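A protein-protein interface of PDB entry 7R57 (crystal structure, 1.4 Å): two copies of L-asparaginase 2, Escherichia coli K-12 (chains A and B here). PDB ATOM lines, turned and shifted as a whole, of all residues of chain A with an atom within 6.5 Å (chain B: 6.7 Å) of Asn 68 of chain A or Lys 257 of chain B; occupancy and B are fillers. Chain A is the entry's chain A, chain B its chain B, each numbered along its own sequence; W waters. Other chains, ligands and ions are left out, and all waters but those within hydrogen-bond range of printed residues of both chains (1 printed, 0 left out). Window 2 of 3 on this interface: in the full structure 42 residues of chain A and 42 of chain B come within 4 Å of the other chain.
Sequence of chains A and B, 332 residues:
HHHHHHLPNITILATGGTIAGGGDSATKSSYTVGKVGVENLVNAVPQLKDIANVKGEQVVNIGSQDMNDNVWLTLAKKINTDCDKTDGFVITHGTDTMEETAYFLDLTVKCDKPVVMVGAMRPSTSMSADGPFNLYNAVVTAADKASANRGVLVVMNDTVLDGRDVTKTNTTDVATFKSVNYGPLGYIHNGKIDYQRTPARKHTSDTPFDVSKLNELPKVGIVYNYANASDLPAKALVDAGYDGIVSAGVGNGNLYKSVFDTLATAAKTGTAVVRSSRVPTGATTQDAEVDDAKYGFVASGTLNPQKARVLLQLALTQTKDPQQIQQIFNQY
Water W1 lies within hydrogen-bond range of OD1 of Asp 66 of chain A (2.6 Å), O of Leu 255 of chain B (2.8 Å) and N of Lys 257 of chain B (3.4 Å).
Printed residues of chain B within 4 Å of Met 67 of chain A: Ala 227 (3.3 Å), Asn 228 (2.9 Å) and Tyr 256 (3.3 Å). Printed residues of chain B within 4 Å of Asn 68 of chain A: Asn 228 (3.3 Å), Tyr 256 (3.99 Å) and Lys 257 (3.6 Å). Printed residues of chain B within 4 Å of Asp 69 of chain A: Asn 228 (2.9 Å). Printed residues of chain B within 4 Å of Arg 309 of chain A: Ala 227 and Asn 228. Of the printed residues of chain A, Asn 228 of chain B touches Met 67, Asn 68, Asp 69 and Arg 309. Of chain A, only Asp 66 and Asn 68 come within 4 Å of Lys 257 of chain B. The nearest printed residue of chain B that does not touch Asn 68 of chain A is Ala 227 of chain B (4.4 Å).
OD1 of Asp 66 of chain A is in hydrogen-bond range of N of Lys 257 of chain B, at 2.9 Å. The backbone NH (N) of Asn 228 of chain B lies within hydrogen-bond range of the backbone carbonyl oxygen (O) of Met 67 of chain A. N of Asp 69 of chain A is in hydrogen-bond range of OD1 of Asn 228 of chain B, 2.9 Å away. The backbone carbonyl oxygen (O) of Ala 227 of chain B is in hydrogen-bond range of the guanidinium group (NH1) of Arg 309 of chain A (3.2 Å).
No position is printed for both chains. Of the 14 pairs that touch across the chains among the printed residues, none has its exchanged pair printed and touching as well.
CG of Gln 65 of chain A touches O of Leu 255 of chain B (3.4 Å). Tyr 256 of chain B touches Gln 65 of chain A. O of Asp 66 of chain A touches CE1 of Tyr 256 of chain B, 3.7 Å away. Met 67 of chain A touches Ala 227 of chain B (O to CA, 3.3 Å). Met 67 of chain A touches Tyr 256 of chain B (O to CE1, 3.3 Å). Asn 68 of chain A touches Asn 228 of chain B (CB to OD1, 3.3 Å). Tyr 256 of chain B touches Asn 68 of chain A. Lys 257 of chain B touches Asn 68 of chain A (NZ to ND2, 3.6 Å). Ala 227 of chain B touches Trp 72 of chain A (CB to CZ2, 3.6 Å). CB of Asn 228 of chain B touches NH2 of Arg 309 of chain A, at 3.4 Å.
The backbone carbonyl oxygen (O) of Asp 66 of chain A lies within hydrogen-bond range of the side-chain amide nitrogen (ND2) of Asn 68 of chain A. NE1 of Trp 72 of chain A sits close to SD of Met 67 of chain A, 3.7 Å away. The backbone NH (N) of Asn 70 of chain A lies within hydrogen-bond range of the side-chain amide oxygen (OD1) of Asn 68 of chain A (3.0 Å). The side-chain carboxylate (OD1) of Asp 69 of chain A is in salt-bridge range of the guanidinium group (NH2) of Arg 309 of chain A, 3.1 Å away. N of Tyr 256 of chain B sits at hydrogen-bond distance from OD1 of Asn 225 of chain B, 3.0 Å away. The side-chain hydroxyl of Tyr 256 of chain B lies within hydrogen-bond range of the side-chain amino group of Lys 257 of chain B (3.0 Å).
Of the 12 printed residues of chain A, 7 touch a printed residue of chain B. Hydrophobic or aromatic side chains of chain A that line the printed part of chain B: Trp 72. Printed residues of chain B that touch a printed residue of chain A: Ala 227, Asn 228, Leu 255, Tyr 256 and Lys 257.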
ATOM      1  N   ILE A  62      18.152  -1.510  26.069  1.00  0.00           N
ATOM      2  CA  ILE A  62      18.056  -1.916  24.677  1.00  0.00           C
ATOM      3  C   ILE A  62      17.219  -0.901  23.923  1.00  0.00           C
ATOM      4  O   ILE A  62      16.401  -0.182  24.501  1.00  0.00           O
ATOM      5  CB  ILE A  62      17.449  -3.319  24.494  1.00  0.00           C
ATOM      6  CG1 ILE A  62      16.057  -3.429  25.099  1.00  0.00           C
ATOM      7  CG2 ILE A  62      18.367  -4.364  25.113  1.00  0.00           C
ATOM      8  CD1 ILE A  62      15.347  -4.648  24.565  1.00  0.00           C
ATOM      9  N   SER A  64      14.066  -0.284  21.669  1.00  0.00           N
ATOM     10  CA  SER A  64      12.819  -1.035  21.730  1.00  0.00           C
ATOM     11  C   SER A  64      12.512  -1.789  20.437  1.00  0.00           C
ATOM     12  O   SER A  64      11.670  -2.690  20.441  1.00  0.00           O
ATOM     13  CB  SER A  64      11.636  -0.145  22.144  1.00  0.00           C
ATOM     14  OG  SER A  64      11.034   0.544  21.053  1.00  0.00           O
ATOM     15  N   GLN A  65      13.187  -1.467  19.327  1.00  0.00           N
ATOM     16  CA  GLN A  65      13.029  -2.332  18.161  1.00  0.00           C
ATOM     17  C   GLN A  65      13.570  -3.733  18.401  1.00  0.00           C
ATOM     18  O   GLN A  65      13.227  -4.640  17.640  1.00  0.00           O
ATOM     19  CB  GLN A  65      13.691  -1.701  16.925  1.00  0.00           C
ATOM     20  CG  GLN A  65      15.218  -1.811  16.888  1.00  0.00           C
ATOM     21  CD  GLN A  65      15.931  -0.838  17.789  1.00  0.00           C
ATOM     22  OE1 GLN A  65      15.330   0.031  18.436  1.00  0.00           O
ATOM     23  NE2 GLN A  65      17.256  -0.979  17.840  1.00  0.00           N
ATOM     24  N   ASP A  66      14.355  -3.927  19.467  1.00  0.00           N
ATOM     25  CA  ASP A  66      14.891  -5.222  19.861  1.00  0.00           C
ATOM     26  C   ASP A  66      14.160  -5.801  21.075  1.00  0.00           C
ATOM     27  O   ASP A  66      14.636  -6.764  21.689  1.00  0.00           O
ATOM     28  CB  ASP A  66      16.403  -5.103  20.153  1.00  0.00           C
ATOM     29  CG  ASP A  66      17.232  -4.809  18.917  1.00  0.00           C
ATOM     30  OD1 ASP A  66      16.824  -5.197  17.804  1.00  0.00           O
ATOM     31  OD2 ASP A  66      18.324  -4.197  19.085  1.00  0.00           O
ATOM     32  N   MET A  67      13.019  -5.222  21.464  1.00  0.00           N
ATOM     33  CA  MET A  67      12.210  -5.774  22.532  1.00  0.00           C
ATOM     34  C   MET A  67      11.884  -7.240  22.279  1.00  0.00           C
ATOM     35  O   MET A  67      11.755  -7.686  21.141  1.00  0.00           O
ATOM     36  CB  MET A  67      10.928  -4.924  22.646  1.00  0.00           C
ATOM     37  CG  MET A  67      10.042  -5.191  23.834  1.00  0.00           C
ATOM     38  SD  MET A  67      10.929  -5.114  25.410  1.00  0.00           S
ATOM     39  CE  MET A  67      11.731  -3.567  25.361  1.00  0.00           C
ATOM     40  N   ASN A  68      11.737  -7.998  23.368  1.00  0.00           N
ATOM     41  CA  ASN A  68      11.572  -9.438  23.240  1.00  0.00           C
ATOM     42  C   ASN A  68      10.901 -10.030  24.478  1.00  0.00           C
ATOM     43  O   ASN A  68      10.680  -9.344  25.482  1.00  0.00           O
ATOM     44  CB  ASN A  68      12.940 -10.088  23.033  1.00  0.00           C
ATOM     45  CG  ASN A  68      13.868  -9.798  24.176  1.00  0.00           C
ATOM     46  OD1 ASN A  68      13.694 -10.352  25.260  1.00  0.00           O
ATOM     47  ND2 ASN A  68      14.783  -8.854  23.996  1.00  0.00           N
ATOM     48  N   ASP A  69      10.579 -11.331  24.379  1.00  0.00           N
ATOM     49  CA  ASP A  69       9.804 -12.031  25.403  1.00  0.00           C
ATOM     50  C   ASP A  69      10.511 -11.997  26.752  1.00  0.00           C
ATOM     51  O   ASP A  69       9.868 -11.951  27.805  1.00  0.00           O
ATOM     52  CB  ASP A  69       9.628 -13.510  25.049  1.00  0.00           C
ATOM     53  CG  ASP A  69       8.744 -13.780  23.843  1.00  0.00           C
ATOM     54  OD1 ASP A  69       8.126 -12.864  23.265  1.00  0.00           O
ATOM     55  OD2 ASP A  69       8.645 -14.977  23.478  1.00  0.00           O
ATOM     56  N   ASN A  70      11.838 -12.091  26.756  1.00  0.00           N
ATOM     57  CA  ASN A  70      12.549 -12.165  28.033  1.00  0.00           C
ATOM     58  C   ASN A  70      12.405 -10.867  28.820  1.00  0.00           C
ATOM     59  O   ASN A  70      12.241 -10.884  30.042  1.00  0.00           O
ATOM     60  CB  ASN A  70      14.027 -12.491  27.806  1.00  0.00           C
ATOM     61  CG  ASN A  70      14.241 -13.883  27.211  1.00  0.00           C
ATOM     62  OD1 ASN A  70      13.469 -14.807  27.451  1.00  0.00           O
ATOM     63  ND2 ASN A  70      15.288 -14.022  26.407  1.00  0.00           N
ATOM     64  N   VAL A  71      12.476  -9.722  28.137  1.00  0.00           N
ATOM     65  CA  VAL A  71      12.283  -8.448  28.819  1.00  0.00           C
ATOM     66  C   VAL A  71      10.855  -8.322  29.336  1.00  0.00           C
ATOM     67  O   VAL A  71      10.628  -7.837  30.442  1.00  0.00           O
ATOM     68  CB  VAL A  71      12.626  -7.296  27.866  1.00  0.00           C
ATOM     69  CG1 VAL A  71      12.304  -5.982  28.535  1.00  0.00           C
ATOM     70  CG2 VAL A  71      14.088  -7.403  27.459  1.00  0.00           C
ATOM     71  N   TRP A  72       9.870  -8.737  28.539  1.00  0.00           N
ATOM     72  CA  TRP A  72       8.483  -8.705  28.985  1.00  0.00           C
ATOM     73  C   TRP A  72       8.325  -9.486  30.275  1.00  0.00           C
ATOM     74  O   TRP A  72       7.723  -9.004  31.235  1.00  0.00           O
ATOM     75  CB  TRP A  72       7.580  -9.265  27.895  1.00  0.00           C
ATOM     76  CG  TRP A  72       7.373  -8.323  26.762  1.00  0.00           C
ATOM     77  CD1 TRP A  72       7.883  -7.085  26.643  1.00  0.00           C
ATOM     78  CD2 TRP A  72       6.611  -8.576  25.589  1.00  0.00           C
ATOM     79  NE1 TRP A  72       7.477  -6.518  25.446  1.00  0.00           N
ATOM     80  CE2 TRP A  72       6.700  -7.422  24.782  1.00  0.00           C
ATOM     81  CE3 TRP A  72       5.882  -9.671  25.125  1.00  0.00           C
ATOM     82  CZ2 TRP A  72       6.064  -7.335  23.541  1.00  0.00           C
ATOM     83  CZ3 TRP A  72       5.221  -9.560  23.919  1.00  0.00           C
ATOM     84  CH2 TRP A  72       5.324  -8.404  23.138  1.00  0.00           C
ATOM     85  N   LEU A  73       8.852 -10.705  30.310  1.00  0.00           N
ATOM     86  CA  LEU A  73       8.732 -11.519  31.519  1.00  0.00           C
ATOM     87  C   LEU A  73       9.437 -10.871  32.700  1.00  0.00           C
ATOM     88  O   LEU A  73       8.906 -10.876  33.823  1.00  0.00           O
ATOM     89  CB  LEU A  73       9.281 -12.921  31.246  1.00  0.00           C
ATOM     90  CG  LEU A  73       8.404 -13.758  30.317  1.00  0.00           C
ATOM     91  CD1 LEU A  73       9.158 -15.013  29.863  1.00  0.00           C
ATOM     92  CD2 LEU A  73       7.090 -14.123  31.013  1.00  0.00           C
ATOM     93  N   ARG A 309      -0.729 -10.632  18.549  1.00  0.00           N
ATOM     94  CA  ARG A 309       0.315 -11.590  18.920  1.00  0.00           C
ATOM     95  C   ARG A 309       0.459 -11.679  20.427  1.00  0.00           C
ATOM     96  O   ARG A 309       0.581 -12.782  20.987  1.00  0.00           O
ATOM     97  CB  ARG A 309       1.652 -11.165  18.321  1.00  0.00           C
ATOM     98  CG  ARG A 309       2.839 -11.961  18.925  1.00  0.00           C
ATOM     99  CD  ARG A 309       4.120 -11.713  18.190  1.00  0.00           C
ATOM    100  NE  ARG A 309       5.206 -12.446  18.846  1.00  0.00           N
ATOM    101  CZ  ARG A 309       5.907 -12.015  19.885  1.00  0.00           C
ATOM    102  NH1 ARG A 309       5.706 -10.831  20.421  1.00  0.00           N
ATOM    103  NH2 ARG A 309       6.834 -12.812  20.425  1.00  0.00           N
ATOM    104  N   ASN B 225       7.798  -6.470  11.229  1.00  0.00           N
ATOM    105  CA  ASN B 225       8.621  -6.343  12.416  1.00  0.00           C
ATOM    106  C   ASN B 225       7.742  -6.084  13.633  1.00  0.00           C
ATOM    107  O   ASN B 225       6.698  -5.406  13.549  1.00  0.00           O
ATOM    108  CB  ASN B 225       9.653  -5.227  12.304  1.00  0.00           C
ATOM    109  CG  ASN B 225      10.752  -5.544  11.313  1.00  0.00           C
ATOM    110  OD1 ASN B 225      11.846  -5.988  11.704  1.00  0.00           O
ATOM    111  ND2 ASN B 225      10.491  -5.299  10.044  1.00  0.00           N
ATOM    112  N   ALA B 227       8.048  -7.125  18.319  1.00  0.00           N
ATOM    113  CA  ALA B 227       8.911  -7.668  19.373  1.00  0.00           C
ATOM    114  C   ALA B 227       9.169  -9.156  19.138  1.00  0.00           C
ATOM    115  O   ALA B 227       8.264  -9.916  18.798  1.00  0.00           O
ATOM    116  CB  ALA B 227       8.244  -7.452  20.719  1.00  0.00           C
ATOM    117  N   ASN B 228      10.445  -9.560  19.302  1.00  0.00           N
ATOM    118  CA  ASN B 228      10.822 -10.983  19.219  1.00  0.00           C
ATOM    119  C   ASN B 228      10.593 -11.566  17.830  1.00  0.00           C
ATOM    120  O   ASN B 228      10.362 -12.760  17.669  1.00  0.00           O
ATOM    121  CB  ASN B 228      10.056 -11.814  20.276  1.00  0.00           C
ATOM    122  CG  ASN B 228      10.892 -12.921  20.904  1.00  0.00           C
ATOM    123  OD1 ASN B 228      11.328 -12.803  22.054  1.00  0.00           O
ATOM    124  ND2 ASN B 228      11.092 -14.001  20.159  1.00  0.00           N
ATOM    125  N   ALA B 229      10.628 -10.741  16.806  1.00  0.00           N
ATOM    126  CA  ALA B 229      10.264 -11.191  15.474  1.00  0.00           C
ATOM    127  C   ALA B 229      11.202 -12.272  14.941  1.00  0.00           C
ATOM    128  O   ALA B 229      12.428 -12.124  14.969  1.00  0.00           O
ATOM    129  CB  ALA B 229      10.286  -9.992  14.524  1.00  0.00           C
ATOM    130  N   LEU B 255      14.230  -2.155  12.474  1.00  0.00           N
ATOM    131  CA  LEU B 255      14.142  -3.592  12.258  1.00  0.00           C
ATOM    132  C   LEU B 255      14.532  -4.332  13.530  1.00  0.00           C
ATOM    133  O   LEU B 255      15.482  -3.941  14.209  1.00  0.00           O
ATOM    134  CB  LEU B 255      15.081  -4.020  11.128  1.00  0.00           C
ATOM    135  CG  LEU B 255      14.694  -3.390   9.779  1.00  0.00           C
ATOM    136  CD1 LEU B 255      15.765  -2.412   9.464  1.00  0.00           C
ATOM    137  CD2 LEU B 255      14.575  -4.448   8.711  1.00  0.00           C
ATOM    138  N   TYR B 256      13.783  -5.385  13.858  1.00  0.00           N
ATOM    139  CA  TYR B 256      14.181  -6.291  14.939  1.00  0.00           C
ATOM    140  C   TYR B 256      15.529  -6.921  14.588  1.00  0.00           C
ATOM    141  O   TYR B 256      15.784  -7.230  13.418  1.00  0.00           O
ATOM    142  CB  TYR B 256      13.119  -7.387  15.124  1.00  0.00           C
ATOM    143  CG  TYR B 256      13.451  -8.311  16.256  1.00  0.00           C
ATOM    144  CD1 TYR B 256      13.345  -7.875  17.554  1.00  0.00           C
ATOM    145  CD2 TYR B 256      13.936  -9.598  16.022  1.00  0.00           C
ATOM    146  CE1 TYR B 256      13.698  -8.680  18.607  1.00  0.00           C
ATOM    147  CE2 TYR B 256      14.265 -10.414  17.081  1.00  0.00           C
ATOM    148  CZ  TYR B 256      14.167  -9.939  18.362  1.00  0.00           C
ATOM    149  OH  TYR B 256      14.509 -10.747  19.428  1.00  0.00           O
ATOM    150  N   LYS B 257      16.377  -7.112  15.607  1.00  0.00           N
ATOM    151  CA  LYS B 257      17.775  -7.518  15.358  1.00  0.00           C
ATOM    152  C   LYS B 257      17.900  -8.700  14.390  1.00  0.00           C
ATOM    153  O   LYS B 257      18.696  -8.647  13.430  1.00  0.00           O
ATOM    154  CB  LYS B 257      18.514  -7.790  16.675  1.00  0.00           C
ATOM    155  CG  LYS B 257      17.881  -8.821  17.592  1.00  0.00           C
ATOM    156  CD  LYS B 257      18.442  -8.730  19.045  1.00  0.00           C
ATOM    157  CE  LYS B 257      17.787  -9.739  20.019  1.00  0.00           C
ATOM    158  NZ  LYS B 257      16.637  -9.204  20.874  1.00  0.00           N
ATOM    159  N   SER B 258      17.123  -9.770  14.593  1.00  0.00           N
ATOM    160  CA  SER B 258      17.298 -10.948  13.741  1.00  0.00           C
ATOM    161  C   SER B 258      16.901 -10.660  12.297  1.00  0.00           C
ATOM    162  O   SER B 258      17.526 -11.167  11.347  1.00  0.00           O
ATOM    163  CB  SER B 258      16.446 -12.096  14.257  1.00  0.00           C
ATOM    164  OG  SER B 258      16.659 -12.273  15.646  1.00  0.00           O
ATOM    165  N   VAL B 259      15.855  -9.848  12.107  1.00  0.00           N
ATOM    166  CA  VAL B 259      15.446  -9.466  10.763  1.00  0.00           C
ATOM    167  C   VAL B 259      16.496  -8.571  10.129  1.00  0.00           C
ATOM    168  O   VAL B 259      16.861  -8.747   8.957  1.00  0.00           O
ATOM    169  CB  VAL B 259      14.071  -8.763  10.825  1.00  0.00           C
ATOM    170  CG1 VAL B 259      13.612  -8.338   9.452  1.00  0.00           C
ATOM    171  CG2 VAL B 259      13.040  -9.681  11.476  1.00  0.00           C
ATOM    172  N   PHE B 260      16.998  -7.602  10.890  1.00  0.00           N
ATOM    173  CA  PHE B 260      18.094  -6.753  10.426  1.00  0.00           C
ATOM    174  C   PHE B 260      19.250  -7.618   9.923  1.00  0.00           C
ATOM    175  O   PHE B 260      19.775  -7.388   8.835  1.00  0.00           O
ATOM    176  CB  PHE B 260      18.533  -5.864  11.591  1.00  0.00           C
ATOM    177  CG  PHE B 260      19.210  -4.575  11.211  1.00  0.00           C
ATOM    178  CD1 PHE B 260      20.037  -4.486  10.129  1.00  0.00           C
ATOM    179  CD2 PHE B 260      19.019  -3.432  11.997  1.00  0.00           C
ATOM    180  CE1 PHE B 260      20.673  -3.288   9.812  1.00  0.00           C
ATOM    181  CE2 PHE B 260      19.636  -2.240  11.689  1.00  0.00           C
ATOM    182  CZ  PHE B 260      20.464  -2.167  10.569  1.00  0.00           C
ATOM    183  N   ASP B 261      19.651  -8.621  10.706  1.00  0.00           N
ATOM    184  CA  ASP B 261      20.822  -9.419  10.327  1.00  0.00           C
ATOM    185  C   ASP B 261      20.596 -10.108   8.989  1.00  0.00           C
ATOM    186  O   ASP B 261      21.498 -10.157   8.141  1.00  0.00           O
ATOM    187  CB  ASP B 261      21.086 -10.464  11.410  1.00  0.00           C
ATOM    188  CG  ASP B 261      21.623  -9.884  12.690  1.00  0.00           C
ATOM    189  OD1 ASP B 261      22.079  -8.730  12.683  1.00  0.00           O
ATOM    190  OD2 ASP B 261      21.598 -10.617  13.714  1.00  0.00           O
ATOM    191  N   THR B 262      19.412 -10.676   8.786  1.00  0.00           N
ATOM    192  CA  THR B 262      19.114 -11.377   7.554  1.00  0.00           C
ATOM    193  C   THR B 262      19.084 -10.425   6.380  1.00  0.00           C
ATOM    194  O   THR B 262      19.587 -10.739   5.293  1.00  0.00           O
ATOM    195  CB  THR B 262      17.796 -12.132   7.693  1.00  0.00           C
ATOM    196  OG1 THR B 262      17.970 -13.164   8.676  1.00  0.00           O
ATOM    197  CG2 THR B 262      17.355 -12.762   6.371  1.00  0.00           C
HETATM  198  O   HOH W   1      17.837  -4.071  15.640  1.00  0.00           O
